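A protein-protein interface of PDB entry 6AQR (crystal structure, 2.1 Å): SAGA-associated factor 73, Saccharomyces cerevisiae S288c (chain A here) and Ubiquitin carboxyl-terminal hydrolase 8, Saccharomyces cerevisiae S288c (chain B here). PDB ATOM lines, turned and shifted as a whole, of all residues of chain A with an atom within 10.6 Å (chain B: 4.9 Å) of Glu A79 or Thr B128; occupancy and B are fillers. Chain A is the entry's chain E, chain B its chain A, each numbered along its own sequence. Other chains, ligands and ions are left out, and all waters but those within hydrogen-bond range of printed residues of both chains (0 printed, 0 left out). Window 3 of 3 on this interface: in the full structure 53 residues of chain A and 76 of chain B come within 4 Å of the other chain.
O of Lys B129 sits at hydrogen-bond distance from N of Glu A79, at 2.8 Å.
The side-chain hydroxyl of Thr B130 lies within hydrogen-bond range of the guanidinium group of Arg A76, 2.7 Å away.
The backbone NH (N) of Val A77 is in hydrogen-bond range of the backbone carbonyl oxygen (O) of Met B131, 2.7 Å away.
The side-chain sulfur of Met B131 lies close to the side-chain carboxylate of Glu A79 (3.6 Å).
The backbone carbonyl oxygen (O) of Asp B124 lies close to the side-chain hydroxyl (OG1) of Thr B128, 3.4 Å away.
The side-chain hydroxyl of Thr B128 lies within hydrogen-bond range of the backbone carbonyl oxygen of Asp B125, at 3.1 Å.
OD1 of Asp B125 lies within salt-bridge range of NZ of Lys B129 (2.9 Å).
The backbone carbonyl oxygen (O) of Val B126 sits at hydrogen-bond distance from the side-chain hydroxyl (OG1) of Thr B130.
The backbone NH (N) of Leu A85 sits at hydrogen-bond distance from the backbone carbonyl oxygen (O) of Arg A76 (2.6 Å).
The side-chain sulfur of Cys A78 lies close to the backbone NH of Lys A80 (3.5 Å).
Of the 8 printed residues of chain B, 7 touch a printed residue of chain A.
Printed residues of chain B that touch a printed residue of chain A: Asp B125, Val B126, Cys B127, Thr B128, Lys B129, Thr B130 and Met B131.
Along chain B the printed residues that touch a printed residue of chain A span positions 125 to 131.
Of the 14 printed residues of chain A, 6 touch a printed residue of chain B.
Among the printed residues, 15 pairs touch across the chains.
CG1 of Val B126 touches NE of Arg A76 (3.8 Å).
CA of Cys B127 touches NH2 of Arg A76, 3.9 Å away.
CA of Arg A76 touches O of Met B131, 3.3 Å away.
Thr B130 touches Val A77.
Lys B129 touches Cys A78 (O to C, 3.7 Å).
Glu A79 touches Thr B128 (CG to O, 3.6 Å).
Thr B130 touches Glu A79 (N to CG, 3.9 Å).
Ile A90 touches Val B126.
Ile A90 touches Thr B130 (CG2 to CG2, 3.9 Å).
Asp B125 touches Leu A94.
Of chain B, only Thr B128, Lys B129, Thr B130 and Met B131 come within 4 Å of Glu A79.
Lys A80 touches none of the printed residues of chain B.
Lys A83 touches none of the printed residues of chain B.
Of the printed residues of chain B, Ile A90 touches Val B126 and Thr B130.
Printed residues of chain A within 4 Å of Val B126: Arg A76 and Ile A90.
Of chain A, only Glu A79 (3.6 Å) comes within 4 Å of Thr B128.
Lys B129 touches just these residues of chain A: Cys A78, Glu A79 and Leu A94.
Met B131 touches just these residues of chain A: Arg A76, Val A77 and Glu A79.
The nearest printed residue of chain B that does not touch Leu A94 is Thr B130 (4.5 Å).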
ATOM      1  N   TYR A  75      20.627  13.212 -15.895  1.00  0.00           N
ATOM      2  CA  TYR A  75      21.169  12.165 -15.055  1.00  0.00           C
ATOM      3  C   TYR A  75      21.508  12.652 -13.683  1.00  0.00           C
ATOM      4  O   TYR A  75      21.588  13.835 -13.463  1.00  0.00           O
ATOM      5  CB  TYR A  75      22.433  11.500 -15.673  1.00  0.00           C
ATOM      6  CG  TYR A  75      23.657  12.386 -15.723  1.00  0.00           C
ATOM      7  CD1 TYR A  75      24.696  12.186 -14.859  1.00  0.00           C
ATOM      8  CD2 TYR A  75      23.806  13.356 -16.727  1.00  0.00           C
ATOM      9  CE1 TYR A  75      25.857  12.945 -14.926  1.00  0.00           C
ATOM     10  CE2 TYR A  75      24.945  14.136 -16.788  1.00  0.00           C
ATOM     11  CZ  TYR A  75      25.976  13.911 -15.889  1.00  0.00           C
ATOM     12  OH  TYR A  75      27.177  14.656 -15.921  1.00  0.00           O
ATOM     13  N   ARG A  76      21.656  11.687 -12.767  1.00  0.00           N
ATOM     14  CA  ARG A  76      22.230  11.949 -11.435  1.00  0.00           C
ATOM     15  C   ARG A  76      23.439  11.009 -11.243  1.00  0.00           C
ATOM     16  O   ARG A  76      23.569  10.002 -11.961  1.00  0.00           O
ATOM     17  CB  ARG A  76      21.147  11.781 -10.340  1.00  0.00           C
ATOM     18  CG  ARG A  76      20.087  12.890 -10.393  1.00  0.00           C
ATOM     19  CD  ARG A  76      18.957  12.642  -9.379  1.00  0.00           C
ATOM     20  NE  ARG A  76      19.461  12.934  -8.001  1.00  0.00           N
ATOM     21  CZ  ARG A  76      19.355  14.098  -7.373  1.00  0.00           C
ATOM     22  NH1 ARG A  76      18.713  15.162  -7.942  1.00  0.00           N
ATOM     23  NH2 ARG A  76      19.831  14.175  -6.114  1.00  0.00           N
ATOM     24  N   VAL A  77      24.336  11.360 -10.314  1.00  0.00           N
ATOM     25  CA  VAL A  77      25.577  10.630 -10.048  1.00  0.00           C
ATOM     26  C   VAL A  77      25.491   9.916  -8.711  1.00  0.00           C
ATOM     27  O   VAL A  77      25.108  10.524  -7.710  1.00  0.00           O
ATOM     28  CB  VAL A  77      26.723  11.638 -10.003  1.00  0.00           C
ATOM     29  CG1 VAL A  77      28.006  11.037  -9.473  1.00  0.00           C
ATOM     30  CG2 VAL A  77      26.889  12.307 -11.361  1.00  0.00           C
ATOM     31  N   CYS A  78      25.834   8.630  -8.712  1.00  0.00           N
ATOM     32  CA  CYS A  78      25.706   7.795  -7.539  1.00  0.00           C
ATOM     33  C   CYS A  78      26.699   8.302  -6.468  1.00  0.00           C
ATOM     34  O   CYS A  78      27.877   8.544  -6.781  1.00  0.00           O
ATOM     35  CB  CYS A  78      26.005   6.330  -7.885  1.00  0.00           C
ATOM     36  SG  CYS A  78      26.095   5.182  -6.446  1.00  0.00           S
ATOM     37  N   GLU A  79      26.220   8.493  -5.234  1.00  0.00           N
ATOM     38  CA  GLU A  79      27.087   8.951  -4.126  1.00  0.00           C
ATOM     39  C   GLU A  79      28.219   7.936  -3.816  1.00  0.00           C
ATOM     40  O   GLU A  79      29.331   8.340  -3.532  1.00  0.00           O
ATOM     41  CB  GLU A  79      26.245   9.181  -2.861  1.00  0.00           C
ATOM     42  CG  GLU A  79      25.341  10.402  -2.912  1.00  0.00           C
ATOM     43  CD  GLU A  79      26.066  11.711  -2.674  1.00  0.00           C
ATOM     44  OE1 GLU A  79      27.152  11.719  -2.060  1.00  0.00           O
ATOM     45  OE2 GLU A  79      25.534  12.754  -3.102  1.00  0.00           O
ATOM     46  N   LYS A  80      27.926   6.636  -3.905  1.00  0.00           N
ATOM     47  CA  LYS A  80      28.898   5.594  -3.603  1.00  0.00           C
ATOM     48  C   LYS A  80      29.905   5.394  -4.715  1.00  0.00           C
ATOM     49  O   LYS A  80      31.086   5.449  -4.448  1.00  0.00           O
ATOM     50  CB  LYS A  80      28.230   4.259  -3.199  1.00  0.00           C
ATOM     51  CG  LYS A  80      27.478   4.260  -1.851  1.00  0.00           C
ATOM     52  CD  LYS A  80      28.100   5.173  -0.764  1.00  0.00           C
ATOM     53  CE  LYS A  80      27.065   5.783   0.201  1.00  0.00           C
ATOM     54  NZ  LYS A  80      26.062   6.758  -0.360  1.00  0.00           N
ATOM     55  N   CYS A  81      29.465   5.156  -5.949  1.00  0.00           N
ATOM     56  CA  CYS A  81      30.433   4.791  -6.999  1.00  0.00           C
ATOM     57  C   CYS A  81      30.758   5.907  -8.011  1.00  0.00           C
ATOM     58  O   CYS A  81      31.634   5.725  -8.857  1.00  0.00           O
ATOM     59  CB  CYS A  81      30.039   3.506  -7.697  1.00  0.00           C
ATOM     60  SG  CYS A  81      28.499   3.637  -8.616  1.00  0.00           S
ATOM     61  N   GLY A  82      30.071   7.050  -7.913  1.00  0.00           N
ATOM     62  CA  GLY A  82      30.262   8.159  -8.869  1.00  0.00           C
ATOM     63  C   GLY A  82      29.813   7.835 -10.312  1.00  0.00           C
ATOM     64  O   GLY A  82      30.096   8.631 -11.201  1.00  0.00           O
ATOM     65  N   LYS A  83      29.081   6.732 -10.538  1.00  0.00           N
ATOM     66  CA  LYS A  83      28.546   6.486 -11.839  1.00  0.00           C
ATOM     67  C   LYS A  83      27.433   7.482 -12.264  1.00  0.00           C
ATOM     68  O   LYS A  83      26.533   7.756 -11.445  1.00  0.00           O
ATOM     69  CB  LYS A  83      28.049   5.067 -11.950  1.00  0.00           C
ATOM     70  CG  LYS A  83      29.092   4.095 -12.458  1.00  0.00           C
ATOM     71  CD  LYS A  83      28.367   2.777 -12.673  1.00  0.00           C
ATOM     72  CE  LYS A  83      29.365   1.684 -13.007  1.00  0.00           C
ATOM     73  NZ  LYS A  83      28.680   0.374 -13.259  1.00  0.00           N
ATOM     74  N   PRO A  84      27.486   8.006 -13.552  1.00  0.00           N
ATOM     75  CA  PRO A  84      26.385   8.788 -14.086  1.00  0.00           C
ATOM     76  C   PRO A  84      25.198   7.899 -14.418  1.00  0.00           C
ATOM     77  O   PRO A  84      25.349   6.968 -15.219  1.00  0.00           O
ATOM     78  CB  PRO A  84      26.968   9.445 -15.352  1.00  0.00           C
ATOM     79  CG  PRO A  84      28.049   8.567 -15.801  1.00  0.00           C
ATOM     80  CD  PRO A  84      28.592   7.883 -14.542  1.00  0.00           C
ATOM     81  N   LEU A  85      24.028   8.198 -13.835  1.00  0.00           N
ATOM     82  CA  LEU A  85      22.803   7.348 -14.022  1.00  0.00           C
ATOM     83  C   LEU A  85      21.647   8.011 -14.662  1.00  0.00           C
ATOM     84  O   LEU A  85      21.216   9.047 -14.209  1.00  0.00           O
ATOM     85  CB  LEU A  85      22.332   6.748 -12.701  1.00  0.00           C
ATOM     86  CG  LEU A  85      23.419   6.148 -11.759  1.00  0.00           C
ATOM     87  CD1 LEU A  85      22.813   5.760 -10.404  1.00  0.00           C
ATOM     88  CD2 LEU A  85      24.188   4.972 -12.379  1.00  0.00           C
ATOM     89  N   ILE A  90      17.997   4.714 -11.956  1.00  0.00           N
ATOM     90  CA  ILE A  90      18.483   5.044 -10.609  1.00  0.00           C
ATOM     91  C   ILE A  90      18.037   4.063  -9.546  1.00  0.00           C
ATOM     92  O   ILE A  90      18.871   3.604  -8.751  1.00  0.00           O
ATOM     93  CB  ILE A  90      18.081   6.471 -10.227  1.00  0.00           C
ATOM     94  CG1 ILE A  90      18.851   7.460 -11.138  1.00  0.00           C
ATOM     95  CG2 ILE A  90      18.306   6.708  -8.728  1.00  0.00           C
ATOM     96  CD1 ILE A  90      18.495   8.927 -10.933  1.00  0.00           C
ATOM     97  N   HIS A  93      19.778   0.696  -9.622  1.00  0.00           N
ATOM     98  CA  HIS A  93      21.199   0.707  -9.320  1.00  0.00           C
ATOM     99  C   HIS A  93      21.391   0.654  -7.807  1.00  0.00           C
ATOM    100  O   HIS A  93      22.372   0.057  -7.302  1.00  0.00           O
ATOM    101  CB  HIS A  93      21.885   1.953  -9.874  1.00  0.00           C
ATOM    102  CG  HIS A  93      23.324   2.059  -9.495  1.00  0.00           C
ATOM    103  ND1 HIS A  93      24.332   1.404 -10.188  1.00  0.00           N
ATOM    104  CD2 HIS A  93      23.928   2.728  -8.479  1.00  0.00           C
ATOM    105  CE1 HIS A  93      25.501   1.701  -9.623  1.00  0.00           C
ATOM    106  NE2 HIS A  93      25.284   2.490  -8.580  1.00  0.00           N
ATOM    107  N   LEU A  94      20.437   1.280  -7.107  1.00  0.00           N
ATOM    108  CA  LEU A  94      20.438   1.400  -5.652  1.00  0.00           C
ATOM    109  C   LEU A  94      20.079   0.044  -4.994  1.00  0.00           C
ATOM    110  O   LEU A  94      19.601  -0.020  -3.860  1.00  0.00           O
ATOM    111  CB  LEU A  94      19.503   2.563  -5.254  1.00  0.00           C
ATOM    112  CG  LEU A  94      19.995   3.924  -5.762  1.00  0.00           C
ATOM    113  CD1 LEU A  94      19.099   5.063  -5.326  1.00  0.00           C
ATOM    114  CD2 LEU A  94      21.461   4.231  -5.480  1.00  0.00           C
ATOM    115  N   ASP B 124      12.699  10.091  -1.999  1.00  0.00           N
ATOM    116  CA  ASP B 124      13.429  10.008  -0.712  1.00  0.00           C
ATOM    117  C   ASP B 124      14.754   9.291  -0.922  1.00  0.00           C
ATOM    118  O   ASP B 124      15.834   9.776  -0.575  1.00  0.00           O
ATOM    119  CB  ASP B 124      12.582   9.253   0.341  1.00  0.00           C
ATOM    120  CG  ASP B 124      11.282  10.039   0.771  1.00  0.00           C
ATOM    121  OD1 ASP B 124      11.217  11.314   0.616  1.00  0.00           O
ATOM    122  OD2 ASP B 124      10.339   9.364   1.294  1.00  0.00           O
ATOM    123  N   ASP B 125      14.656   8.129  -1.540  1.00  0.00           N
ATOM    124  CA  ASP B 125      15.797   7.337  -1.767  1.00  0.00           C
ATOM    125  C   ASP B 125      16.709   7.974  -2.833  1.00  0.00           C
ATOM    126  O   ASP B 125      17.937   7.994  -2.669  1.00  0.00           O
ATOM    127  CB  ASP B 125      15.317   5.952  -2.185  1.00  0.00           C
ATOM    128  CG  ASP B 125      16.394   4.914  -2.053  1.00  0.00           C
ATOM    129  OD1 ASP B 125      17.108   4.922  -0.995  1.00  0.00           O
ATOM    130  OD2 ASP B 125      16.524   4.100  -3.016  1.00  0.00           O
ATOM    131  N   VAL B 126      16.117   8.522  -3.907  1.00  0.00           N
ATOM    132  CA  VAL B 126      16.907   9.168  -4.996  1.00  0.00           C
ATOM    133  C   VAL B 126      17.815  10.327  -4.521  1.00  0.00           C
ATOM    134  O   VAL B 126      19.010  10.345  -4.862  1.00  0.00           O
ATOM    135  CB  VAL B 126      16.008   9.531  -6.204  1.00  0.00           C
ATOM    136  CG1 VAL B 126      16.748  10.368  -7.226  1.00  0.00           C
ATOM    137  CG2 VAL B 126      15.480   8.237  -6.850  1.00  0.00           C
ATOM    138  N   CYS B 127      17.273  11.250  -3.726  1.00  0.00           N
ATOM    139  CA  CYS B 127      18.016  12.397  -3.181  1.00  0.00           C
ATOM    140  C   CYS B 127      19.200  12.059  -2.327  1.00  0.00           C
ATOM    141  O   CYS B 127      20.213  12.755  -2.369  1.00  0.00           O
ATOM    142  CB  CYS B 127      17.122  13.254  -2.280  1.00  0.00           C
ATOM    143  SG  CYS B 127      15.886  14.094  -3.232  1.00  0.00           S
ATOM    144  N   THR B 128      19.042  11.033  -1.502  1.00  0.00           N
ATOM    145  CA  THR B 128      20.048  10.698  -0.507  1.00  0.00           C
ATOM    146  C   THR B 128      21.194   9.918  -1.166  1.00  0.00           C
ATOM    147  O   THR B 128      22.338  10.190  -0.872  1.00  0.00           O
ATOM    148  CB  THR B 128      19.447   9.927   0.680  1.00  0.00           C
ATOM    149  OG1 THR B 128      18.955   8.652   0.225  1.00  0.00           O
ATOM    150  CG2 THR B 128      18.311  10.720   1.295  1.00  0.00           C
ATOM    151  N   LYS B 129      20.881   9.009  -2.092  1.00  0.00           N
ATOM    152  CA  LYS B 129      21.890   8.157  -2.729  1.00  0.00           C
ATOM    153  C   LYS B 129      22.540   8.718  -4.000  1.00  0.00           C
ATOM    154  O   LYS B 129      23.558   8.210  -4.433  1.00  0.00           O
ATOM    155  CB  LYS B 129      21.268   6.805  -3.064  1.00  0.00           C
ATOM    156  CG  LYS B 129      20.597   6.103  -1.882  1.00  0.00           C
ATOM    157  CD  LYS B 129      21.581   5.502  -0.873  1.00  0.00           C
ATOM    158  CE  LYS B 129      20.877   5.131   0.427  1.00  0.00           C
ATOM    159  NZ  LYS B 129      19.651   4.327   0.159  1.00  0.00           N
ATOM    160  N   THR B 130      21.925   9.735  -4.622  1.00  0.00           N
ATOM    161  CA  THR B 130      22.457  10.306  -5.878  1.00  0.00           C
ATOM    162  C   THR B 130      22.503  11.793  -5.746  1.00  0.00           C
ATOM    163  O   THR B 130      21.680  12.364  -5.054  1.00  0.00           O
ATOM    164  CB  THR B 130      21.629   9.904  -7.130  1.00  0.00           C
ATOM    165  OG1 THR B 130      20.330  10.498  -7.108  1.00  0.00           O
ATOM    166  CG2 THR B 130      21.492   8.393  -7.242  1.00  0.00           C
ATOM    167  N   MET B 131      23.425  12.425  -6.445  1.00  0.00           N
ATOM    168  CA  MET B 131      23.518  13.894  -6.489  1.00  0.00           C
ATOM    169  C   MET B 131      23.445  14.382  -7.938  1.00  0.00           C
ATOM    170  O   MET B 131      23.510  13.543  -8.897  1.00  0.00           O
ATOM    171  CB  MET B 131      24.831  14.346  -5.877  1.00  0.00           C
ATOM    172  CG  MET B 131      26.018  13.674  -6.561  1.00  0.00           C
ATOM    173  SD  MET B 131      27.597  14.052  -5.814  1.00  0.00           S
ATOM    174  CE  MET B 131      28.339  15.272  -6.940  1.00  0.00           C
